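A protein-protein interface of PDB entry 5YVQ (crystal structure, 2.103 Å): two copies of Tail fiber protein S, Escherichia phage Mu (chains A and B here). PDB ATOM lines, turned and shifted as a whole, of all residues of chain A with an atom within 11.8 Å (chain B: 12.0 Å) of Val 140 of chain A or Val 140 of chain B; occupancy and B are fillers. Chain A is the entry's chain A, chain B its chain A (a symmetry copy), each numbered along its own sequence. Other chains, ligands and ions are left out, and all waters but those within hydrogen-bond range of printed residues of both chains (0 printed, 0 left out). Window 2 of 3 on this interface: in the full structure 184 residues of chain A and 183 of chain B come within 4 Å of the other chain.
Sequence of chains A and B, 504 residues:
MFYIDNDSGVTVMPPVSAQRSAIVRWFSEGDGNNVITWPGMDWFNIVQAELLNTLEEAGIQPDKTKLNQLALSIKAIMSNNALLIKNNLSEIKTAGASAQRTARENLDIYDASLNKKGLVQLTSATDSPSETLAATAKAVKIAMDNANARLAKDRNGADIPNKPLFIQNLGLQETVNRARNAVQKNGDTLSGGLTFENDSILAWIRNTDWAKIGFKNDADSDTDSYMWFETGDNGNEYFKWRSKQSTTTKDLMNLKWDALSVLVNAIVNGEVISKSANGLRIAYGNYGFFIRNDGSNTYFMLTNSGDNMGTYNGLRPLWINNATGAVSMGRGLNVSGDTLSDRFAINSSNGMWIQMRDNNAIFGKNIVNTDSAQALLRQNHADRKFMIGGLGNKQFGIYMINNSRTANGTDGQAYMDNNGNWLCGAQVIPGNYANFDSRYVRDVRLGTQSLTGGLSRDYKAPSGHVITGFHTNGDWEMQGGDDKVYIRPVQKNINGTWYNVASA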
ATOM      1  N   LYS A 138      14.411  31.031 -37.392  1.00  0.00           N
ATOM      2  CA  LYS A 138      14.802  29.788 -36.742  1.00  0.00           C
ATOM      3  C   LYS A 138      14.433  29.794 -35.263  1.00  0.00           C
ATOM      4  O   LYS A 138      14.817  28.891 -34.521  1.00  0.00           O
ATOM      5  CB  LYS A 138      16.306  29.542 -36.897  1.00  0.00           C
ATOM      6  CG  LYS A 138      16.717  28.962 -38.243  1.00  0.00           C
ATOM      7  CD  LYS A 138      18.002  28.156 -38.137  1.00  0.00           C
ATOM      8  CE  LYS A 138      18.456  27.648 -39.495  1.00  0.00           C
ATOM      9  NZ  LYS A 138      17.319  27.098 -40.283  1.00  0.00           N
ATOM     10  N   ALA A 139      13.692  30.817 -34.832  1.00  0.00           N
ATOM     11  CA  ALA A 139      13.221  30.847 -33.451  1.00  0.00           C
ATOM     12  C   ALA A 139      12.230  29.722 -33.173  1.00  0.00           C
ATOM     13  O   ALA A 139      12.200  29.185 -32.061  1.00  0.00           O
ATOM     14  CB  ALA A 139      12.590  32.201 -33.133  1.00  0.00           C
ATOM     15  N   VAL A 140      11.411  29.358 -34.162  1.00  0.00           N
ATOM     16  CA  VAL A 140      10.517  28.213 -34.025  1.00  0.00           C
ATOM     17  C   VAL A 140      11.227  26.879 -34.235  1.00  0.00           C
ATOM     18  O   VAL A 140      10.705  25.836 -33.814  1.00  0.00           O
ATOM     19  CB  VAL A 140       9.329  28.343 -34.995  1.00  0.00           C
ATOM     20  CG1 VAL A 140       9.731  27.889 -36.393  1.00  0.00           C
ATOM     21  CG2 VAL A 140       8.129  27.534 -34.492  1.00  0.00           C
ATOM     22  N   LYS A 141      12.396  26.879 -34.876  1.00  0.00           N
ATOM     23  CA  LYS A 141      13.181  25.657 -34.972  1.00  0.00           C
ATOM     24  C   LYS A 141      13.604  25.177 -33.589  1.00  0.00           C
ATOM     25  O   LYS A 141      13.665  23.969 -33.334  1.00  0.00           O
ATOM     26  CB  LYS A 141      14.395  25.893 -35.867  1.00  0.00           C
ATOM     27  CG  LYS A 141      15.408  24.776 -35.874  1.00  0.00           C
ATOM     28  CD  LYS A 141      16.485  25.045 -36.906  1.00  0.00           C
ATOM     29  CE  LYS A 141      17.678  24.128 -36.712  1.00  0.00           C
ATOM     30  NZ  LYS A 141      18.380  24.428 -35.435  1.00  0.00           N
ATOM     31  N   ILE A 142      13.883  26.112 -32.677  1.00  0.00           N
ATOM     32  CA  ILE A 142      14.178  25.743 -31.296  1.00  0.00           C
ATOM     33  C   ILE A 142      12.955  25.099 -30.651  1.00  0.00           C
ATOM     34  O   ILE A 142      13.067  24.105 -29.919  1.00  0.00           O
ATOM     35  CB  ILE A 142      14.667  26.973 -30.505  1.00  0.00           C
ATOM     36  CG1 ILE A 142      16.197  27.051 -30.518  1.00  0.00           C
ATOM     37  CG2 ILE A 142      14.160  26.942 -29.070  1.00  0.00           C
ATOM     38  CD1 ILE A 142      16.805  27.307 -31.889  1.00  0.00           C
ATOM     39  N   ALA A 143      11.767  25.641 -30.927  1.00  0.00           N
ATOM     40  CA  ALA A 143      10.544  25.015 -30.438  1.00  0.00           C
ATOM     41  C   ALA A 143      10.291  23.675 -31.118  1.00  0.00           C
ATOM     42  O   ALA A 143       9.788  22.741 -30.481  1.00  0.00           O
ATOM     43  CB  ALA A 143       9.355  25.952 -30.641  1.00  0.00           C
ATOM     44  N   MET A 144      10.637  23.563 -32.403  1.00  0.00           N
ATOM     45  CA  MET A 144      10.466  22.305 -33.121  1.00  0.00           C
ATOM     46  C   MET A 144      11.433  21.243 -32.615  1.00  0.00           C
ATOM     47  O   MET A 144      11.051  20.079 -32.441  1.00  0.00           O
ATOM     48  CB  MET A 144      10.667  22.529 -34.616  1.00  0.00           C
ATOM     49  CG  MET A 144      10.278  21.357 -35.483  1.00  0.00           C
ATOM     50  SD  MET A 144       8.493  21.161 -35.564  1.00  0.00           S
ATOM     51  CE  MET A 144       8.357  19.920 -36.848  1.00  0.00           C
ATOM     52  N   ASP A 145      12.693  21.619 -32.390  1.00  0.00           N
ATOM     53  CA  ASP A 145      13.669  20.664 -31.879  1.00  0.00           C
ATOM     54  C   ASP A 145      13.316  20.223 -30.466  1.00  0.00           C
ATOM     55  O   ASP A 145      13.506  19.055 -30.106  1.00  0.00           O
ATOM     56  CB  ASP A 145      15.066  21.278 -31.919  1.00  0.00           C
ATOM     57  CG  ASP A 145      15.635  21.337 -33.320  1.00  0.00           C
ATOM     58  OD1 ASP A 145      14.956  20.885 -34.267  1.00  0.00           O
ATOM     59  OD2 ASP A 145      16.766  21.838 -33.472  1.00  0.00           O
ATOM     60  N   ASN A 146      12.805  21.149 -29.652  1.00  0.00           N
ATOM     61  CA  ASN A 146      12.352  20.799 -28.313  1.00  0.00           C
ATOM     62  C   ASN A 146      11.249  19.749 -28.374  1.00  0.00           C
ATOM     63  O   ASN A 146      11.316  18.726 -27.684  1.00  0.00           O
ATOM     64  CB  ASN A 146      11.875  22.051 -27.581  1.00  0.00           C
ATOM     65  CG  ASN A 146      11.518  21.785 -26.136  1.00  0.00           C
ATOM     66  OD1 ASN A 146      11.842  20.729 -25.585  1.00  0.00           O
ATOM     67  ND2 ASN A 146      10.850  22.743 -25.509  1.00  0.00           N
ATOM     68  N   ALA A 147      10.230  19.979 -29.207  1.00  0.00           N
ATOM     69  CA  ALA A 147       9.174  18.983 -29.359  1.00  0.00           C
ATOM     70  C   ALA A 147       9.731  17.666 -29.888  1.00  0.00           C
ATOM     71  O   ALA A 147       9.296  16.587 -29.472  1.00  0.00           O
ATOM     72  CB  ALA A 147       8.072  19.511 -30.276  1.00  0.00           C
ATOM     73  N   ASN A 148      10.708  17.734 -30.795  1.00  0.00           N
ATOM     74  CA  ASN A 148      11.277  16.514 -31.355  1.00  0.00           C
ATOM     75  C   ASN A 148      12.063  15.711 -30.323  1.00  0.00           C
ATOM     76  O   ASN A 148      12.316  14.525 -30.547  1.00  0.00           O
ATOM     77  CB  ASN A 148      12.173  16.852 -32.548  1.00  0.00           C
ATOM     78  CG  ASN A 148      11.391  16.992 -33.845  1.00  0.00           C
ATOM     79  OD1 ASN A 148      10.160  16.957 -33.853  1.00  0.00           O
ATOM     80  ND2 ASN A 148      12.108  17.148 -34.951  1.00  0.00           N
ATOM     81  N   ALA A 149      12.455  16.333 -29.213  1.00  0.00           N
ATOM     82  CA  ALA A 149      13.195  15.681 -28.143  1.00  0.00           C
ATOM     83  C   ALA A 149      12.279  15.013 -27.118  1.00  0.00           C
ATOM     84  O   ALA A 149      12.744  14.638 -26.035  1.00  0.00           O
ATOM     85  CB  ALA A 149      14.106  16.695 -27.443  1.00  0.00           C
ATOM     86  N   LYS B 138       5.622  36.179 -28.737  1.00  0.00           N
ATOM     87  CA  LYS B 138       5.414  35.165 -27.713  1.00  0.00           C
ATOM     88  C   LYS B 138       4.454  34.081 -28.190  1.00  0.00           C
ATOM     89  O   LYS B 138       4.045  33.224 -27.409  1.00  0.00           O
ATOM     90  CB  LYS B 138       4.881  35.795 -26.422  1.00  0.00           C
ATOM     91  CG  LYS B 138       5.942  36.450 -25.552  1.00  0.00           C
ATOM     92  CD  LYS B 138       5.536  36.461 -24.085  1.00  0.00           C
ATOM     93  CE  LYS B 138       6.558  37.189 -23.229  1.00  0.00           C
ATOM     94  NZ  LYS B 138       7.950  36.807 -23.592  1.00  0.00           N
ATOM     95  N   ALA B 139       4.089  34.125 -29.473  1.00  0.00           N
ATOM     96  CA  ALA B 139       3.246  33.070 -30.028  1.00  0.00           C
ATOM     97  C   ALA B 139       3.968  31.728 -30.048  1.00  0.00           C
ATOM     98  O   ALA B 139       3.335  30.682 -29.865  1.00  0.00           O
ATOM     99  CB  ALA B 139       2.781  33.444 -31.434  1.00  0.00           C
ATOM    100  N   VAL B 140       5.283  31.734 -30.272  1.00  0.00           N
ATOM    101  CA  VAL B 140       6.074  30.511 -30.188  1.00  0.00           C
ATOM    102  C   VAL B 140       6.406  30.119 -28.751  1.00  0.00           C
ATOM    103  O   VAL B 140       6.753  28.954 -28.501  1.00  0.00           O
ATOM    104  CB  VAL B 140       7.365  30.651 -31.015  1.00  0.00           C
ATOM    105  CG1 VAL B 140       8.422  31.414 -30.227  1.00  0.00           C
ATOM    106  CG2 VAL B 140       7.893  29.273 -31.429  1.00  0.00           C
ATOM    107  N   LYS B 141       6.318  31.053 -27.805  1.00  0.00           N
ATOM    108  CA  LYS B 141       6.482  30.696 -26.403  1.00  0.00           C
ATOM    109  C   LYS B 141       5.392  29.727 -25.963  1.00  0.00           C
ATOM    110  O   LYS B 141       5.639  28.828 -25.151  1.00  0.00           O
ATOM    111  CB  LYS B 141       6.474  31.959 -25.545  1.00  0.00           C
ATOM    112  CG  LYS B 141       6.414  31.718 -24.058  1.00  0.00           C
ATOM    113  CD  LYS B 141       6.567  33.024 -23.304  1.00  0.00           C
ATOM    114  CE  LYS B 141       6.182  32.867 -21.844  1.00  0.00           C
ATOM    115  NZ  LYS B 141       4.728  32.588 -21.702  1.00  0.00           N
ATOM    116  N   ILE B 142       4.179  29.883 -26.504  1.00  0.00           N
ATOM    117  CA  ILE B 142       3.112  28.926 -26.230  1.00  0.00           C
ATOM    118  C   ILE B 142       3.478  27.556 -26.789  1.00  0.00           C
ATOM    119  O   ILE B 142       3.248  26.521 -26.148  1.00  0.00           O
ATOM    120  CB  ILE B 142       1.773  29.443 -26.796  1.00  0.00           C
ATOM    121  CG1 ILE B 142       0.989  30.202 -25.721  1.00  0.00           C
ATOM    122  CG2 ILE B 142       0.931  28.299 -27.344  1.00  0.00           C
ATOM    123  CD1 ILE B 142       1.644  31.495 -25.257  1.00  0.00           C
ATOM    124  N   ALA B 143       4.070  27.527 -27.986  1.00  0.00           N
ATOM    125  CA  ALA B 143       4.549  26.264 -28.535  1.00  0.00           C
ATOM    126  C   ALA B 143       5.728  25.718 -27.739  1.00  0.00           C
ATOM    127  O   ALA B 143       5.854  24.498 -27.575  1.00  0.00           O
ATOM    128  CB  ALA B 143       4.930  26.440 -30.003  1.00  0.00           C
ATOM    129  N   MET B 144       6.592  26.603 -27.234  1.00  0.00           N
ATOM    130  CA  MET B 144       7.727  26.171 -26.426  1.00  0.00           C
ATOM    131  C   MET B 144       7.270  25.625 -25.079  1.00  0.00           C
ATOM    132  O   MET B 144       7.785  24.601 -24.611  1.00  0.00           O
ATOM    133  CB  MET B 144       8.692  27.333 -26.222  1.00  0.00           C
ATOM    134  CG  MET B 144      10.017  26.948 -25.612  1.00  0.00           C
ATOM    135  SD  MET B 144      11.047  26.053 -26.783  1.00  0.00           S
ATOM    136  CE  MET B 144      12.594  25.998 -25.883  1.00  0.00           C
ATOM    137  N   ASP B 145       6.319  26.302 -24.434  1.00  0.00           N
ATOM    138  CA  ASP B 145       5.815  25.826 -23.152  1.00  0.00           C
ATOM    139  C   ASP B 145       5.072  24.507 -23.312  1.00  0.00           C
ATOM    140  O   ASP B 145       5.160  23.628 -22.445  1.00  0.00           O
ATOM    141  CB  ASP B 145       4.907  26.882 -22.527  1.00  0.00           C
ATOM    142  CG  ASP B 145       5.681  28.050 -21.956  1.00  0.00           C
ATOM    143  OD1 ASP B 145       6.929  28.039 -22.027  1.00  0.00           O
ATOM    144  OD2 ASP B 145       5.037  28.982 -21.436  1.00  0.00           O
ATOM    145  N   ASN B 146       4.335  24.355 -24.413  1.00  0.00           N
ATOM    146  CA  ASN B 146       3.665  23.095 -24.697  1.00  0.00           C
ATOM    147  C   ASN B 146       4.676  21.958 -24.802  1.00  0.00           C
ATOM    148  O   ASN B 146       4.513  20.910 -24.168  1.00  0.00           O
ATOM    149  CB  ASN B 146       2.845  23.217 -25.980  1.00  0.00           C
ATOM    150  CG  ASN B 146       2.013  21.987 -26.263  1.00  0.00           C
ATOM    151  OD1 ASN B 146       1.840  21.122 -25.399  1.00  0.00           O
ATOM    152  ND2 ASN B 146       1.485  21.901 -27.476  1.00  0.00           N
ATOM    153  N   ALA B 147       5.737  22.154 -25.590  1.00  0.00           N
ATOM    154  CA  ALA B 147       6.774  21.130 -25.684  1.00  0.00           C
ATOM    155  C   ALA B 147       7.422  20.877 -24.328  1.00  0.00           C
ATOM    156  O   ALA B 147       7.742  19.733 -23.988  1.00  0.00           O
ATOM    157  CB  ALA B 147       7.823  21.529 -26.719  1.00  0.00           C
ATOM    158  N   ASN B 148       7.608  21.932 -23.531  1.00  0.00           N
ATOM    159  CA  ASN B 148       8.236  21.764 -22.226  1.00  0.00           C
ATOM    160  C   ASN B 148       7.363  20.974 -21.256  1.00  0.00           C
ATOM    161  O   ASN B 148       7.876  20.475 -20.252  1.00  0.00           O
ATOM    162  CB  ASN B 148       8.577  23.131 -21.629  1.00  0.00           C
ATOM    163  CG  ASN B 148       9.914  23.666 -22.119  1.00  0.00           C
ATOM    164  OD1 ASN B 148      10.548  23.084 -23.000  1.00  0.00           O
ATOM    165  ND2 ASN B 148      10.349  24.781 -21.543  1.00  0.00           N
ATOM    166  N   ALA B 149       6.065  20.861 -21.533  1.00  0.00           N
ATOM    167  CA  ALA B 149       5.126  20.121 -20.702  1.00  0.00           C
ATOM    168  C   ALA B 149       5.055  18.641 -21.072  1.00  0.00           C
ATOM    169  O   ALA B 149       4.134  17.943 -20.629  1.00  0.00           O
ATOM    170  CB  ALA B 149       3.732  20.750 -20.801  1.00  0.00           C
ATOM    171  N   ARG B 150       6.008  18.153 -21.863  1.00  0.00           N
ATOM    172  CA  ARG B 150       5.968  16.816 -22.424  1.00  0.00           C
ATOM    173  C   ARG B 150       7.194  16.024 -21.990  1.00  0.00           C
ATOM    174  O   ARG B 150       8.254  16.596 -21.707  1.00  0.00           O
ATOM    175  CB  ARG B 150       5.881  16.865 -23.953  1.00  0.00           C
ATOM    176  CG  ARG B 150       4.477  16.675 -24.483  1.00  0.00           C
ATOM    177  CD  ARG B 150       3.839  17.978 -24.895  1.00  0.00           C
ATOM    178  NE  ARG B 150       2.559  17.763 -25.559  1.00  0.00           N
ATOM    179  CZ  ARG B 150       1.384  18.132 -25.058  1.00  0.00           C
ATOM    180  NH1 ARG B 150       1.327  18.745 -23.882  1.00  0.00           N
ATOM    181  NH2 ARG B 150       0.266  17.896 -25.736  1.00  0.00           N
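Hydrophobic or aromatic side chains of chain B that line the printed part of chain A: Val 140, Met 144 and Ala 147.
CG2 of Val 140 of chain B touches CG2 of Val 140 of chain A, 3.5 Å away. Ile 142 of chain A touches Met 144 of chain B (CG2 to CE, 3.7 Å). Ala 143 of chain A touches Val 140 of chain B (CB to CG2, 3.7 Å). Ala 143 of chain A touches Met 144 of chain B. Ala 147 of chain B touches Asn 146 of chain A (CB to ND2, 3.5 Å). Ala 147 of chain B touches Ala 147 of chain A (CB to N, 3.8 Å).
Ile 142 of chain A touches Met 144 of chain B, but with the chains exchanged Met 144 of chain A does not touch Ile 142 of chain B (9.9 Å). Ala 143 of chain A touches Val 140 of chain B, but with the chains exchanged Val 140 of chain A does not touch Ala 143 of chain B (5.6 Å). Asn 146 of chain A touches Met 144 of chain B, but with the chains exchanged Met 144 of chain A does not touch Asn 146 of chain B (9.8 Å). Asn 146 of chain A touches Ala 147 of chain B, but with the chains exchanged Ala 147 of chain A does not touch Asn 146 of chain B (6.9 Å). 12 positions are printed for both chains. Of the 8 pairs that touch across the chains among the printed residues, 2 have their exchanged pair printed and touching as well.
No residue of chain B comes within 4 Å of Ala 139 of chain A. Of the printed residues of chain B, Val 140 of chain A touches Val 140. No residue of chain B comes within 4 Å of Lys 141 of chain A. Ile 142 of chain A touches just one residue of chain B: Met 144. Ala 143 of chain A touches two residues of chain B. No residue of chain B comes within 4 Å of Met 144 of chain A. Printed residues of chain B within 4 Å of Asn 146 of chain A: Met 144, Ala 147 and Asn 148. Of the printed residues of chain B, Ala 147 of chain A touches Ala 147 (3.8 Å). No residue of chain A comes within 4 Å of Ala 139 of chain B. Of chain A, only Val 140 and Ala 143 come within 4 Å of Val 140 of chain B. No residue of chain A comes within 4 Å of Lys 141 of chain B. No residue of chain A comes within 4 Å of Ile 142 of chain B. No residue of chain A comes within 4 Å of Ala 143 of chain B. Met 144 of chain B touches three residues of chain A. Asp 145 of chain B touches none of the printed residues of chain A. Arg 150 of chain B touches none of the printed residues of chain A. The nearest residue of chain B that does not touch Val 140 of chain A is Ala 143 of chain B (5.6 Å). The nearest printed residue of chain B that does not touch Asn 146 of chain A is Ala 143 of chain B (5.7 Å).
The side-chain amide nitrogen (ND2) of Asn 146 of chain A is in hydrogen-bond range of the side-chain sulfur (SD) of Met 144 of chain B (3.6 Å). OD1 of Asn 148 of chain B lies within hydrogen-bond range of ND2 of Asn 146 of chain A, 2.6 Å away.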
